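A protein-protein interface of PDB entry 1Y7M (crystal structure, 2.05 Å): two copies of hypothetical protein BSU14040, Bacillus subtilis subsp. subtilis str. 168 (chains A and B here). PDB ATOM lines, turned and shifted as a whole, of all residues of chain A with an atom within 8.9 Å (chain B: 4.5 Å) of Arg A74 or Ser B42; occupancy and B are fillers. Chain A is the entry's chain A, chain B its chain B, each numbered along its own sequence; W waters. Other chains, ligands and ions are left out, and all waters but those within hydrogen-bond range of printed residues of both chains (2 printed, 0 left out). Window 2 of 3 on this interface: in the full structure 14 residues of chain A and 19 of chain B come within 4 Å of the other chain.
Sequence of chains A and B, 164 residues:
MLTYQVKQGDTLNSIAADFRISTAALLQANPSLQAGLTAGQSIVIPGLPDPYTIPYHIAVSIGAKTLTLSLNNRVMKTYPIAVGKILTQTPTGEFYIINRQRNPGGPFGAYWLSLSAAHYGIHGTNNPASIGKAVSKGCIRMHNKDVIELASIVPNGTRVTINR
Water W1 bridges N of Gln B5 and OD1 of Asn A73. Water W2 lies within hydrogen-bond range of OD1 of Asn A73 (3.2 Å) and NE2 of Gln B5 (3.4 Å).
O of Gly B40 lies within hydrogen-bond range of N of Val A75, 2.8 Å away. ND2 of Asn A73 is in hydrogen-bond range of OG1 of Thr B3, at 2.7 Å. The backbone carbonyl oxygen (O) of Gln B41 sits close to the backbone carbonyl oxygen (O) of Asn A73 (3.2 Å). The backbone carbonyl oxygen (O) of Asn A73 sits close to the backbone NH (N) of Ser B42, at 3.4 Å. The side-chain hydroxyl (OG) of Ser A70 is in hydrogen-bond range of the side-chain amide nitrogen (NE2) of Gln B5 (2.8 Å).
No position is printed for both chains.
Arg A74 touches just these residues of chain B: Gln B5, Gly B40 and Ser B42. Ser B42 touches just these residues of chain A: Asn A72 (3.6 Å), Asn A73 (3.3 Å) and Arg A74 (3.7 Å). Of the printed residues of chain B, Asn A72 touches Ser B42. Of the printed residues of chain A, Gln B41 touches Asn A73. Printed residues of chain B within 4 Å of Val A75: Gln B5 and Gly B40. Of the printed residues of chain A, Gly B40 touches Asn A73, Arg A74 and Val A75. Thr A68 touches none of the printed residues of chain B. The nearest printed residue of chain A that does not touch Tyr B4 is Asn A72 (6.3 Å).
Asn A72 touches Ser B42. ND2 of Asn A73 touches N of Tyr B4, 3.7 Å away. Asn A73 touches Gln B5. O of Gly B40 touches O of Asn A73, 3.7 Å away. Gln B5 touches Arg A74. O of Gly B40 touches CA of Arg A74, 3.2 Å away. Arg A74 touches Ser B42 (CG to N, 3.7 Å). OE1 of Gln B5 touches CG1 of Val A75, at 3.98 Å.
Printed residues of chain B that touch a printed residue of chain A: Thr B3, Tyr B4, Gln B5, Gly B40, Gln B41 and Ser B42.
The backbone NH (N) of Ser A70 lies within hydrogen-bond range of the backbone carbonyl oxygen (O) of His A57, 2.9 Å away. The backbone NH of Tyr B4 sits at hydrogen-bond distance from the backbone carbonyl oxygen of Ile B43 (3.0 Å). NH1 of Arg A74 is in hydrogen-bond range of O of Asn A72 (3.3 Å). O of Pro A55 lies within hydrogen-bond range of N of Asn A72, at 2.9 Å.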
ATOM      1  N   PRO A  55      31.521 -20.974  11.839  1.00  0.00           N
ATOM      2  CA  PRO A  55      31.008 -22.203  12.469  1.00  0.00           C
ATOM      3  C   PRO A  55      30.356 -21.948  13.843  1.00  0.00           C
ATOM      4  O   PRO A  55      29.815 -22.885  14.450  1.00  0.00           O
ATOM      5  CB  PRO A  55      32.265 -23.069  12.608  1.00  0.00           C
ATOM      6  CG  PRO A  55      33.411 -22.048  12.744  1.00  0.00           C
ATOM      7  CD  PRO A  55      32.986 -20.871  11.954  1.00  0.00           C
ATOM      8  N   TYR A  56      30.394 -20.706  14.313  1.00  0.00           N
ATOM      9  CA  TYR A  56      29.703 -20.324  15.521  1.00  0.00           C
ATOM     10  C   TYR A  56      28.258 -19.961  15.231  1.00  0.00           C
ATOM     11  O   TYR A  56      27.920 -19.464  14.160  1.00  0.00           O
ATOM     12  CB  TYR A  56      30.388 -19.148  16.220  1.00  0.00           C
ATOM     13  CG  TYR A  56      31.766 -19.473  16.742  1.00  0.00           C
ATOM     14  CD1 TYR A  56      32.896 -19.053  16.056  1.00  0.00           C
ATOM     15  CD2 TYR A  56      31.937 -20.216  17.914  1.00  0.00           C
ATOM     16  CE1 TYR A  56      34.169 -19.344  16.520  1.00  0.00           C
ATOM     17  CE2 TYR A  56      33.216 -20.517  18.394  1.00  0.00           C
ATOM     18  CZ  TYR A  56      34.330 -20.069  17.681  1.00  0.00           C
ATOM     19  OH  TYR A  56      35.603 -20.351  18.113  1.00  0.00           O
ATOM     20  N   HIS A  57      27.421 -20.227  16.214  1.00  0.00           N
ATOM     21  CA  HIS A  57      26.004 -19.965  16.134  1.00  0.00           C
ATOM     22  C   HIS A  57      25.565 -19.681  17.563  1.00  0.00           C
ATOM     23  O   HIS A  57      25.757 -20.511  18.447  1.00  0.00           O
ATOM     24  CB  HIS A  57      25.255 -21.195  15.568  1.00  0.00           C
ATOM     25  CG  HIS A  57      23.857 -20.897  15.129  1.00  0.00           C
ATOM     26  ND1 HIS A  57      23.405 -21.176  13.866  1.00  0.00           N
ATOM     27  CD2 HIS A  57      22.816 -20.328  15.781  1.00  0.00           C
ATOM     28  CE1 HIS A  57      22.149 -20.775  13.749  1.00  0.00           C
ATOM     29  NE2 HIS A  57      21.766 -20.258  14.899  1.00  0.00           N
ATOM     30  N   THR A  68      23.278 -19.427  24.368  1.00  0.00           N
ATOM     31  CA  THR A  68      24.089 -20.607  24.140  1.00  0.00           C
ATOM     32  C   THR A  68      24.980 -20.427  22.908  1.00  0.00           C
ATOM     33  O   THR A  68      24.488 -20.122  21.823  1.00  0.00           O
ATOM     34  CB  THR A  68      23.155 -21.838  23.991  1.00  0.00           C
ATOM     35  OG1 THR A  68      22.298 -21.939  25.139  1.00  0.00           O
ATOM     36  CG2 THR A  68      23.931 -23.113  24.081  1.00  0.00           C
ATOM     37  N   LEU A  69      26.285 -20.590  23.086  1.00  0.00           N
ATOM     38  CA  LEU A  69      27.220 -20.588  21.968  1.00  0.00           C
ATOM     39  C   LEU A  69      27.537 -22.004  21.511  1.00  0.00           C
ATOM     40  O   LEU A  69      27.961 -22.854  22.317  1.00  0.00           O
ATOM     41  CB  LEU A  69      28.516 -19.897  22.376  1.00  0.00           C
ATOM     42  CG  LEU A  69      29.599 -19.809  21.312  1.00  0.00           C
ATOM     43  CD1 LEU A  69      29.144 -18.919  20.152  1.00  0.00           C
ATOM     44  CD2 LEU A  69      30.878 -19.280  21.962  1.00  0.00           C
ATOM     45  N   SER A  70      27.320 -22.246  20.220  1.00  0.00           N
ATOM     46  CA  SER A  70      27.660 -23.511  19.580  1.00  0.00           C
ATOM     47  C   SER A  70      28.823 -23.330  18.601  1.00  0.00           C
ATOM     48  O   SER A  70      29.071 -22.236  18.074  1.00  0.00           O
ATOM     49  CB  SER A  70      26.454 -24.078  18.849  1.00  0.00           C
ATOM     50  OG  SER A  70      25.372 -24.251  19.725  1.00  0.00           O
ATOM     51  N   LEU A  71      29.550 -24.418  18.408  1.00  0.00           N
ATOM     52  CA  LEU A  71      30.631 -24.509  17.447  1.00  0.00           C
ATOM     53  C   LEU A  71      30.368 -25.736  16.625  1.00  0.00           C
ATOM     54  O   LEU A  71      30.280 -26.820  17.195  1.00  0.00           O
ATOM     55  CB  LEU A  71      31.940 -24.681  18.187  1.00  0.00           C
ATOM     56  CG  LEU A  71      33.246 -24.226  17.543  1.00  0.00           C
ATOM     57  CD1 LEU A  71      34.391 -25.112  17.957  1.00  0.00           C
ATOM     58  CD2 LEU A  71      33.195 -24.078  16.057  1.00  0.00           C
ATOM     59  N   ASN A  72      30.233 -25.588  15.307  1.00  0.00           N
ATOM     60  CA  ASN A  72      29.943 -26.738  14.422  1.00  0.00           C
ATOM     61  C   ASN A  72      28.870 -27.690  14.976  1.00  0.00           C
ATOM     62  O   ASN A  72      29.071 -28.906  15.055  1.00  0.00           O
ATOM     63  CB  ASN A  72      31.231 -27.505  14.068  1.00  0.00           C
ATOM     64  CG  ASN A  72      32.181 -26.672  13.180  1.00  0.00           C
ATOM     65  OD1 ASN A  72      31.808 -26.281  12.080  1.00  0.00           O
ATOM     66  ND2 ASN A  72      33.390 -26.381  13.673  1.00  0.00           N
ATOM     67  N   ASN A  73      27.736 -27.101  15.347  1.00  0.00           N
ATOM     68  CA  ASN A  73      26.545 -27.807  15.852  1.00  0.00           C
ATOM     69  C   ASN A  73      26.709 -28.602  17.187  1.00  0.00           C
ATOM     70  O   ASN A  73      25.992 -29.592  17.449  1.00  0.00           O
ATOM     71  CB  ASN A  73      25.941 -28.669  14.733  1.00  0.00           C
ATOM     72  CG  ASN A  73      25.159 -27.841  13.711  1.00  0.00           C
ATOM     73  OD1 ASN A  73      24.478 -26.861  14.054  1.00  0.00           O
ATOM     74  ND2 ASN A  73      25.242 -28.250  12.452  1.00  0.00           N
ATOM     75  N   ARG A  74      27.654 -28.151  18.013  1.00  0.00           N
ATOM     76  CA  ARG A  74      27.872 -28.626  19.383  1.00  0.00           C
ATOM     77  C   ARG A  74      27.854 -27.435  20.329  1.00  0.00           C
ATOM     78  O   ARG A  74      28.638 -26.478  20.136  1.00  0.00           O
ATOM     79  CB  ARG A  74      29.268 -29.256  19.529  1.00  0.00           C
ATOM     80  CG  ARG A  74      29.406 -30.768  19.292  1.00  0.00           C
ATOM     81  CD  ARG A  74      30.876 -31.241  19.345  1.00  0.00           C
ATOM     82  NE  ARG A  74      31.273 -32.271  18.370  1.00  0.00           N
ATOM     83  CZ  ARG A  74      31.513 -32.081  17.061  1.00  0.00           C
ATOM     84  NH1 ARG A  74      31.360 -30.890  16.483  1.00  0.00           N
ATOM     85  NH2 ARG A  74      31.889 -33.111  16.307  1.00  0.00           N
ATOM     86  N   VAL A  75      27.035 -27.476  21.381  1.00  0.00           N
ATOM     87  CA  VAL A  75      27.063 -26.365  22.332  1.00  0.00           C
ATOM     88  C   VAL A  75      28.359 -26.433  23.124  1.00  0.00           C
ATOM     89  O   VAL A  75      28.826 -27.510  23.503  1.00  0.00           O
ATOM     90  CB  VAL A  75      25.767 -26.174  23.240  1.00  0.00           C
ATOM     91  CG1 VAL A  75      24.605 -26.974  22.753  1.00  0.00           C
ATOM     92  CG2 VAL A  75      26.023 -26.414  24.705  1.00  0.00           C
ATOM     93  N   MET A  76      28.937 -25.252  23.303  1.00  0.00           N
ATOM     94  CA  MET A  76      30.223 -25.044  23.917  1.00  0.00           C
ATOM     95  C   MET A  76      30.061 -24.416  25.287  1.00  0.00           C
ATOM     96  O   MET A  76      30.698 -24.833  26.243  1.00  0.00           O
ATOM     97  CB  MET A  76      30.997 -24.057  23.062  1.00  0.00           C
ATOM     98  CG  MET A  76      32.272 -24.529  22.519  1.00  0.00           C
ATOM     99  SD  MET A  76      32.942 -22.965  21.526  1.00  0.00           S
ATOM    100  CE  MET A  76      34.083 -22.268  22.952  1.00  0.00           C
ATOM    101  N   LYS A  77      29.236 -23.376  25.359  1.00  0.00           N
ATOM    102  CA  LYS A  77      29.029 -22.624  26.595  1.00  0.00           C
ATOM    103  C   LYS A  77      27.593 -22.111  26.659  1.00  0.00           C
ATOM    104  O   LYS A  77      27.018 -21.714  25.645  1.00  0.00           O
ATOM    105  CB  LYS A  77      29.996 -21.433  26.663  1.00  0.00           C
ATOM    106  CG  LYS A  77      30.881 -21.397  27.931  1.00  0.00           C
ATOM    107  CD  LYS A  77      30.047 -21.337  29.239  1.00  0.00           C
ATOM    108  CE  LYS A  77      30.667 -20.461  30.370  1.00  0.00           C
ATOM    109  NZ  LYS A  77      32.078 -19.973  30.167  1.00  0.00           N
ATOM    110  N   THR B   3      25.996 -31.806   9.237  1.00  0.00           N
ATOM    111  CA  THR B   3      25.811 -31.951  10.682  1.00  0.00           C
ATOM    112  C   THR B   3      24.498 -31.351  11.138  1.00  0.00           C
ATOM    113  O   THR B   3      23.877 -30.547  10.436  1.00  0.00           O
ATOM    114  CB  THR B   3      26.936 -31.308  11.506  1.00  0.00           C
ATOM    115  OG1 THR B   3      26.969 -29.899  11.270  1.00  0.00           O
ATOM    116  CG2 THR B   3      28.300 -31.818  11.096  1.00  0.00           C
ATOM    117  N   TYR B   4      24.114 -31.745  12.350  1.00  0.00           N
ATOM    118  CA  TYR B   4      22.852 -31.359  12.951  1.00  0.00           C
ATOM    119  C   TYR B   4      23.011 -31.267  14.477  1.00  0.00           C
ATOM    120  O   TYR B   4      23.526 -32.195  15.109  1.00  0.00           O
ATOM    121  CB  TYR B   4      21.788 -32.397  12.576  1.00  0.00           C
ATOM    122  CG  TYR B   4      20.449 -32.192  13.231  1.00  0.00           C
ATOM    123  CD1 TYR B   4      19.577 -31.202  12.778  1.00  0.00           C
ATOM    124  CD2 TYR B   4      20.047 -32.994  14.294  1.00  0.00           C
ATOM    125  CE1 TYR B   4      18.334 -31.009  13.380  1.00  0.00           C
ATOM    126  CE2 TYR B   4      18.814 -32.818  14.904  1.00  0.00           C
ATOM    127  CZ  TYR B   4      17.958 -31.824  14.450  1.00  0.00           C
ATOM    128  OH  TYR B   4      16.732 -31.647  15.062  1.00  0.00           O
ATOM    129  N   GLN B   5      22.592 -30.143  15.060  1.00  0.00           N
ATOM    130  CA  GLN B   5      22.569 -29.992  16.519  1.00  0.00           C
ATOM    131  C   GLN B   5      21.281 -30.584  17.053  1.00  0.00           C
ATOM    132  O   GLN B   5      20.190 -30.154  16.693  1.00  0.00           O
ATOM    133  CB  GLN B   5      22.678 -28.526  16.957  1.00  0.00           C
ATOM    134  CG  GLN B   5      22.671 -28.348  18.485  1.00  0.00           C
ATOM    135  CD  GLN B   5      23.058 -26.944  18.932  1.00  0.00           C
ATOM    136  OE1 GLN B   5      22.279 -26.271  19.604  1.00  0.00           O
ATOM    137  NE2 GLN B   5      24.256 -26.509  18.578  1.00  0.00           N
ATOM    138  N   LEU B  33      28.059 -42.945  18.559  1.00  0.00           N
ATOM    139  CA  LEU B  33      27.853 -42.407  19.904  1.00  0.00           C
ATOM    140  C   LEU B  33      26.372 -42.357  20.329  1.00  0.00           C
ATOM    141  O   LEU B  33      26.066 -41.978  21.463  1.00  0.00           O
ATOM    142  CB  LEU B  33      28.522 -41.019  20.036  1.00  0.00           C
ATOM    143  CG  LEU B  33      27.835 -39.696  19.635  1.00  0.00           C
ATOM    144  CD1 LEU B  33      28.870 -38.681  19.113  1.00  0.00           C
ATOM    145  CD2 LEU B  33      26.715 -39.838  18.608  1.00  0.00           C
ATOM    146  N   GLY B  40      22.203 -30.780  22.396  1.00  0.00           N
ATOM    147  CA  GLY B  40      23.360 -29.900  22.310  1.00  0.00           C
ATOM    148  C   GLY B  40      24.552 -30.466  21.546  1.00  0.00           C
ATOM    149  O   GLY B  40      25.442 -29.704  21.097  1.00  0.00           O
ATOM    150  N   GLN B  41      24.561 -31.789  21.380  1.00  0.00           N
ATOM    151  CA  GLN B  41      25.611 -32.507  20.650  1.00  0.00           C
ATOM    152  C   GLN B  41      25.420 -32.426  19.136  1.00  0.00           C
ATOM    153  O   GLN B  41      24.335 -32.118  18.641  1.00  0.00           O
ATOM    154  CB  GLN B  41      25.626 -34.002  21.050  1.00  0.00           C
ATOM    155  CG  GLN B  41      24.941 -34.950  20.028  1.00  0.00           C
ATOM    156  CD  GLN B  41      24.920 -36.421  20.469  1.00  0.00           C
ATOM    157  OE1 GLN B  41      25.966 -37.088  20.520  1.00  0.00           O
ATOM    158  NE2 GLN B  41      23.735 -36.922  20.768  1.00  0.00           N
ATOM    159  N   SER B  42      26.468 -32.808  18.420  1.00  0.00           N
ATOM    160  CA  SER B  42      26.435 -32.897  16.973  1.00  0.00           C
ATOM    161  C   SER B  42      26.339 -34.343  16.502  1.00  0.00           C
ATOM    162  O   SER B  42      27.040 -35.228  17.006  1.00  0.00           O
ATOM    163  CB  SER B  42      27.691 -32.263  16.383  1.00  0.00           C
ATOM    164  OG  SER B  42      27.566 -32.165  14.984  1.00  0.00           O
ATOM    165  N   ILE B  43      25.460 -34.566  15.531  1.00  0.00           N
ATOM    166  CA  ILE B  43      25.388 -35.834  14.818  1.00  0.00           C
ATOM    167  C   ILE B  43      25.519 -35.541  13.326  1.00  0.00           C
ATOM    168  O   ILE B  43      25.233 -34.425  12.882  1.00  0.00           O
ATOM    169  CB  ILE B  43      24.066 -36.561  15.105  1.00  0.00           C
ATOM    170  CG1 ILE B  43      22.869 -35.754  14.589  1.00  0.00           C
ATOM    171  CG2 ILE B  43      23.928 -36.859  16.605  1.00  0.00           C
ATOM    172  CD1 ILE B  43      21.576 -36.544  14.680  1.00  0.00           C
HETATM  173  O   HOH W   1      21.348 -28.030  13.284  1.00  0.00           O
HETATM  174  O   HOH W   2      24.399 -24.255  15.985  1.00  0.00           O
